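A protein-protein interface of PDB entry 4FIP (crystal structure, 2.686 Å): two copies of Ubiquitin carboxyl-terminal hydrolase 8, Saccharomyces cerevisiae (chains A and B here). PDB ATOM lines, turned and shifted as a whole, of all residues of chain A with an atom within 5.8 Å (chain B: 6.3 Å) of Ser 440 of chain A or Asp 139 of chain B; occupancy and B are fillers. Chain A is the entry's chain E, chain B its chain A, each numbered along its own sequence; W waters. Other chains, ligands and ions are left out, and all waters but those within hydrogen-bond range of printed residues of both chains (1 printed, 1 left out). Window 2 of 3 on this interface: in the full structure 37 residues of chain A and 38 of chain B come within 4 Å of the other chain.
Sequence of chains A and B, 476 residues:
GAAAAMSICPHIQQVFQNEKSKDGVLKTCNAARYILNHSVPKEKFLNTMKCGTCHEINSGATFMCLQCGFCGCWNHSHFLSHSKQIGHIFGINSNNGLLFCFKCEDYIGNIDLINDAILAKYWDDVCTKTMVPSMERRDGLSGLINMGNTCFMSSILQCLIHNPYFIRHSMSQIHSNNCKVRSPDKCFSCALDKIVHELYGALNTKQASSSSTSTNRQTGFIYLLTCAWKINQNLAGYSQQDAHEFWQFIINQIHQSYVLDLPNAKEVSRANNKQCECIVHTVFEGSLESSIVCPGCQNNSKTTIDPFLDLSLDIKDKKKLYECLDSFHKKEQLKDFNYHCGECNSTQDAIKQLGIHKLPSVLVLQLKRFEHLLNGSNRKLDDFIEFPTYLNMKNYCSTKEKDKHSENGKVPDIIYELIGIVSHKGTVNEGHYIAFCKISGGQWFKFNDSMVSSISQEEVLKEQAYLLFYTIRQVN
Water W1 bridges NE2 of His 162 of chain A and O of Gly 140 of chain B.
Printed residues of chain A that touch a printed residue of chain B: His 162, Leu 199, Tyr 200, Ile 439 and Ser 440. Hydrophobic or aromatic side chains of chain B that line the printed part of chain A: Leu 141. Among the printed residues, 11 pairs touch across the chains. Among the printed residues, no Asp or Glu carboxylate lies within 4 Å of a Lys or Arg side-chain nitrogen of the other chain.
Of the printed residues of chain B, His 162 of chain A touches Asp 139 (3.4 Å), Gly 140 (3.7 Å) and Leu 141 (3.8 Å). Of the printed residues of chain B, Tyr 200 of chain A touches Arg 137 (3.7 Å), Asp 139 (3.7 Å) and Gly 140 (3.5 Å). Ser 440 of chain A touches just one residue of chain B: Asp 139 (3.5 Å). Gln 443 of chain A touches none of the printed residues of chain B. The nearest residue of chain B that does not touch Ser 440 of chain A is Arg 138 of chain B (6.2 Å). The nearest printed residue of chain A that does not touch Leu 141 of chain B is Leu 199 of chain A (4.8 Å).
No position is printed for both chains. Of the 11 pairs that touch across the chains among the printed residues, none has its exchanged pair printed and touching as well.
The guanidinium group of Arg 137 of chain B lies within hydrogen-bond range of the backbone carbonyl oxygen of Leu 199 of chain A (3.4 Å).
O of Asp 139 of chain B touches CE1 of His 162 of chain A, 3.4 Å away. His 162 of chain A touches Gly 140 of chain B. Leu 141 of chain B touches His 162 of chain A (CD2 to CE1, 3.8 Å). Gly 140 of chain B touches Leu 199 of chain A (O to CD2, 3.5 Å). Arg 137 of chain B touches Tyr 200 of chain A (CB to O, 3.7 Å). Tyr 200 of chain A touches Asp 139 of chain B (CE1 to C, 3.7 Å). Gly 140 of chain B touches Tyr 200 of chain A (N to CE1, 3.5 Å). Ile 439 of chain A touches Asp 139 of chain B (CD1 to CB, 3.6 Å). Ile 439 of chain A touches Leu 141 of chain B (CD1 to CD1, 3.8 Å). OG of Ser 440 of chain A touches OD1 of Asp 139 of chain B, at 3.5 Å.
OG of Ser 134 of chain B lies close to N of Arg 137 of chain B (3.4 Å). OD2 of Asp 139 of chain B is in salt-bridge range of NE of Arg 138 of chain B (3.8 Å).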
ATOM      1  N   HIS A 162     -19.811 -26.406  -1.468  1.00  0.00           N
ATOM      2  CA  HIS A 162     -18.827 -27.307  -2.084  1.00  0.00           C
ATOM      3  C   HIS A 162     -18.902 -27.271  -3.593  1.00  0.00           C
ATOM      4  O   HIS A 162     -18.215 -28.019  -4.260  1.00  0.00           O
ATOM      5  CB  HIS A 162     -18.945 -28.718  -1.478  1.00  0.00           C
ATOM      6  CG  HIS A 162     -18.526 -28.777  -0.026  1.00  0.00           C
ATOM      7  ND1 HIS A 162     -17.254 -28.988   0.348  1.00  0.00           N
ATOM      8  CD2 HIS A 162     -19.233 -28.525   1.142  1.00  0.00           C
ATOM      9  CE1 HIS A 162     -17.157 -28.919   1.686  1.00  0.00           C
ATOM     10  NE2 HIS A 162     -18.371 -28.646   2.174  1.00  0.00           N
ATOM     11  N   LEU A 199     -15.989 -21.279   7.014  1.00  0.00           N
ATOM     12  CA  LEU A 199     -15.604 -22.633   6.666  1.00  0.00           C
ATOM     13  C   LEU A 199     -14.218 -22.708   6.090  1.00  0.00           C
ATOM     14  O   LEU A 199     -13.522 -23.719   6.272  1.00  0.00           O
ATOM     15  CB  LEU A 199     -16.594 -23.270   5.691  1.00  0.00           C
ATOM     16  CG  LEU A 199     -17.767 -23.992   6.365  1.00  0.00           C
ATOM     17  CD1 LEU A 199     -18.401 -23.074   7.392  1.00  0.00           C
ATOM     18  CD2 LEU A 199     -18.803 -24.448   5.351  1.00  0.00           C
ATOM     19  N   TYR A 200     -13.825 -21.655   5.387  1.00  0.00           N
ATOM     20  CA  TYR A 200     -12.610 -21.693   4.590  1.00  0.00           C
ATOM     21  C   TYR A 200     -11.525 -20.765   5.092  1.00  0.00           C
ATOM     22  O   TYR A 200     -10.381 -20.995   4.816  1.00  0.00           O
ATOM     23  CB  TYR A 200     -12.929 -21.293   3.163  1.00  0.00           C
ATOM     24  CG  TYR A 200     -13.618 -22.338   2.318  1.00  0.00           C
ATOM     25  CD1 TYR A 200     -12.888 -23.298   1.633  1.00  0.00           C
ATOM     26  CD2 TYR A 200     -14.985 -22.326   2.152  1.00  0.00           C
ATOM     27  CE1 TYR A 200     -13.506 -24.253   0.855  1.00  0.00           C
ATOM     28  CE2 TYR A 200     -15.604 -23.268   1.357  1.00  0.00           C
ATOM     29  CZ  TYR A 200     -14.867 -24.234   0.707  1.00  0.00           C
ATOM     30  OH  TYR A 200     -15.500 -25.188  -0.084  1.00  0.00           O
ATOM     31  N   LYS A 438     -18.554 -34.438  -3.355  1.00  0.00           N
ATOM     32  CA  LYS A 438     -17.192 -34.719  -3.773  1.00  0.00           C
ATOM     33  C   LYS A 438     -16.354 -33.455  -3.519  1.00  0.00           C
ATOM     34  O   LYS A 438     -16.729 -32.356  -3.915  1.00  0.00           O
ATOM     35  CB  LYS A 438     -17.181 -35.089  -5.255  1.00  0.00           C
ATOM     36  CG  LYS A 438     -16.237 -36.200  -5.654  1.00  0.00           C
ATOM     37  CD  LYS A 438     -15.887 -36.155  -7.142  1.00  0.00           C
ATOM     38  CE  LYS A 438     -16.385 -37.349  -7.933  1.00  0.00           C
ATOM     39  NZ  LYS A 438     -15.295 -37.831  -8.836  1.00  0.00           N
ATOM     40  N   ILE A 439     -15.238 -33.587  -2.817  1.00  0.00           N
ATOM     41  CA  ILE A 439     -14.260 -32.487  -2.778  1.00  0.00           C
ATOM     42  C   ILE A 439     -13.027 -32.814  -3.650  1.00  0.00           C
ATOM     43  O   ILE A 439     -12.857 -33.950  -4.139  1.00  0.00           O
ATOM     44  CB  ILE A 439     -13.859 -32.070  -1.339  1.00  0.00           C
ATOM     45  CG1 ILE A 439     -12.990 -33.121  -0.670  1.00  0.00           C
ATOM     46  CG2 ILE A 439     -15.096 -31.796  -0.493  1.00  0.00           C
ATOM     47  CD1 ILE A 439     -12.547 -32.645   0.688  1.00  0.00           C
ATOM     48  N   SER A 440     -12.201 -31.796  -3.872  1.00  0.00           N
ATOM     49  CA  SER A 440     -11.036 -31.940  -4.741  1.00  0.00           C
ATOM     50  C   SER A 440     -10.265 -33.225  -4.421  1.00  0.00           C
ATOM     51  O   SER A 440     -10.160 -33.646  -3.267  1.00  0.00           O
ATOM     52  CB  SER A 440     -10.129 -30.720  -4.582  1.00  0.00           C
ATOM     53  OG  SER A 440     -10.044 -30.358  -3.203  1.00  0.00           O
ATOM     54  N   GLY A 441      -9.749 -33.870  -5.451  1.00  0.00           N
ATOM     55  CA  GLY A 441      -9.009 -35.100  -5.250  1.00  0.00           C
ATOM     56  C   GLY A 441      -9.887 -36.325  -5.160  1.00  0.00           C
ATOM     57  O   GLY A 441      -9.376 -37.441  -5.226  1.00  0.00           O
ATOM     58  N   GLY A 442     -11.197 -36.131  -4.970  1.00  0.00           N
ATOM     59  CA  GLY A 442     -12.187 -37.200  -5.163  1.00  0.00           C
ATOM     60  C   GLY A 442     -12.813 -37.812  -3.924  1.00  0.00           C
ATOM     61  O   GLY A 442     -13.526 -38.818  -4.028  1.00  0.00           O
ATOM     62  N   GLN A 443     -12.559 -37.241  -2.752  1.00  0.00           N
ATOM     63  CA  GLN A 443     -13.180 -37.759  -1.540  1.00  0.00           C
ATOM     64  C   GLN A 443     -14.592 -37.269  -1.472  1.00  0.00           C
ATOM     65  O   GLN A 443     -14.859 -36.131  -1.775  1.00  0.00           O
ATOM     66  CB  GLN A 443     -12.501 -37.271  -0.275  1.00  0.00           C
ATOM     67  CG  GLN A 443     -11.451 -38.185   0.312  1.00  0.00           C
ATOM     68  CD  GLN A 443     -10.316 -37.358   0.894  1.00  0.00           C
ATOM     69  OE1 GLN A 443      -9.591 -36.695   0.146  1.00  0.00           O
ATOM     70  NE2 GLN A 443     -10.183 -37.352   2.222  1.00  0.00           N
ATOM     71  N   SER B 134      -5.181 -22.739   6.465  1.00  0.00           N
ATOM     72  CA  SER B 134      -4.954 -23.723   7.493  1.00  0.00           C
ATOM     73  C   SER B 134      -5.405 -25.095   7.007  1.00  0.00           C
ATOM     74  O   SER B 134      -6.319 -25.243   6.203  1.00  0.00           O
ATOM     75  CB  SER B 134      -5.697 -23.367   8.761  1.00  0.00           C
ATOM     76  OG  SER B 134      -7.027 -23.760   8.616  1.00  0.00           O
ATOM     77  N   MET B 135      -4.727 -26.096   7.526  1.00  0.00           N
ATOM     78  CA  MET B 135      -4.935 -27.465   7.140  1.00  0.00           C
ATOM     79  C   MET B 135      -6.362 -27.883   7.377  1.00  0.00           C
ATOM     80  O   MET B 135      -6.888 -28.648   6.607  1.00  0.00           O
ATOM     81  CB  MET B 135      -4.012 -28.324   7.985  1.00  0.00           C
ATOM     82  CG  MET B 135      -4.276 -29.819   7.922  1.00  0.00           C
ATOM     83  SD  MET B 135      -3.108 -30.698   8.970  1.00  0.00           S
ATOM     84  CE  MET B 135      -3.448 -29.927  10.562  1.00  0.00           C
ATOM     85  N   GLU B 136      -6.973 -27.393   8.457  1.00  0.00           N
ATOM     86  CA  GLU B 136      -8.304 -27.850   8.882  1.00  0.00           C
ATOM     87  C   GLU B 136      -9.447 -27.257   8.071  1.00  0.00           C
ATOM     88  O   GLU B 136     -10.500 -27.867   7.996  1.00  0.00           O
ATOM     89  CB  GLU B 136      -8.560 -27.480  10.333  1.00  0.00           C
ATOM     90  CG  GLU B 136      -7.605 -28.113  11.346  1.00  0.00           C
ATOM     91  CD  GLU B 136      -6.335 -27.297  11.579  1.00  0.00           C
ATOM     92  OE1 GLU B 136      -5.397 -27.849  12.207  1.00  0.00           O
ATOM     93  OE2 GLU B 136      -6.260 -26.121  11.124  1.00  0.00           O
ATOM     94  N   ARG B 137      -9.244 -26.059   7.503  1.00  0.00           N
ATOM     95  CA  ARG B 137     -10.265 -25.328   6.769  1.00  0.00           C
ATOM     96  C   ARG B 137     -10.099 -25.447   5.251  1.00  0.00           C
ATOM     97  O   ARG B 137     -10.938 -25.002   4.507  1.00  0.00           O
ATOM     98  CB  ARG B 137     -10.188 -23.841   7.107  1.00  0.00           C
ATOM     99  CG  ARG B 137      -9.941 -23.487   8.563  1.00  0.00           C
ATOM    100  CD  ARG B 137     -11.221 -23.267   9.325  1.00  0.00           C
ATOM    101  NE  ARG B 137     -12.062 -24.451   9.211  1.00  0.00           N
ATOM    102  CZ  ARG B 137     -12.187 -25.407  10.130  1.00  0.00           C
ATOM    103  NH1 ARG B 137     -11.534 -25.343  11.299  1.00  0.00           N
ATOM    104  NH2 ARG B 137     -12.990 -26.436   9.873  1.00  0.00           N
ATOM    105  N   ARG B 138      -9.026 -26.049   4.781  1.00  0.00           N
ATOM    106  CA  ARG B 138      -8.644 -25.918   3.371  1.00  0.00           C
ATOM    107  C   ARG B 138      -9.665 -26.431   2.394  1.00  0.00           C
ATOM    108  O   ARG B 138      -9.658 -26.017   1.230  1.00  0.00           O
ATOM    109  CB  ARG B 138      -7.339 -26.648   3.088  1.00  0.00           C
ATOM    110  CG  ARG B 138      -7.384 -28.134   3.343  1.00  0.00           C
ATOM    111  CD  ARG B 138      -5.987 -28.725   3.377  1.00  0.00           C
ATOM    112  NE  ARG B 138      -6.008 -30.122   2.975  1.00  0.00           N
ATOM    113  CZ  ARG B 138      -6.072 -31.174   3.785  1.00  0.00           C
ATOM    114  NH1 ARG B 138      -6.097 -31.041   5.109  1.00  0.00           N
ATOM    115  NH2 ARG B 138      -6.124 -32.397   3.247  1.00  0.00           N
ATOM    116  N   ASP B 139     -10.492 -27.373   2.838  1.00  0.00           N
ATOM    117  CA  ASP B 139     -11.517 -27.934   1.983  1.00  0.00           C
ATOM    118  C   ASP B 139     -12.908 -27.501   2.418  1.00  0.00           C
ATOM    119  O   ASP B 139     -13.881 -27.976   1.869  1.00  0.00           O
ATOM    120  CB  ASP B 139     -11.376 -29.460   1.926  1.00  0.00           C
ATOM    121  CG  ASP B 139     -10.111 -29.893   1.164  1.00  0.00           C
ATOM    122  OD1 ASP B 139      -9.814 -29.240   0.134  1.00  0.00           O
ATOM    123  OD2 ASP B 139      -9.414 -30.854   1.585  1.00  0.00           O
ATOM    124  N   GLY B 140     -13.005 -26.592   3.388  1.00  0.00           N
ATOM    125  CA  GLY B 140     -14.317 -26.137   3.875  1.00  0.00           C
ATOM    126  C   GLY B 140     -15.198 -27.148   4.613  1.00  0.00           C
ATOM    127  O   GLY B 140     -16.402 -26.919   4.762  1.00  0.00           O
ATOM    128  N   LEU B 141     -14.609 -28.241   5.093  1.00  0.00           N
ATOM    129  CA  LEU B 141     -15.375 -29.321   5.711  1.00  0.00           C
ATOM    130  C   LEU B 141     -15.769 -28.996   7.143  1.00  0.00           C
ATOM    131  O   LEU B 141     -14.923 -28.870   8.005  1.00  0.00           O
ATOM    132  CB  LEU B 141     -14.581 -30.605   5.702  1.00  0.00           C
ATOM    133  CG  LEU B 141     -14.369 -31.188   4.313  1.00  0.00           C
ATOM    134  CD1 LEU B 141     -13.315 -32.270   4.372  1.00  0.00           C
ATOM    135  CD2 LEU B 141     -15.651 -31.730   3.697  1.00  0.00           C
HETATM  136  O   HOH W   1     -18.579 -28.359   4.612  1.00  0.00           O
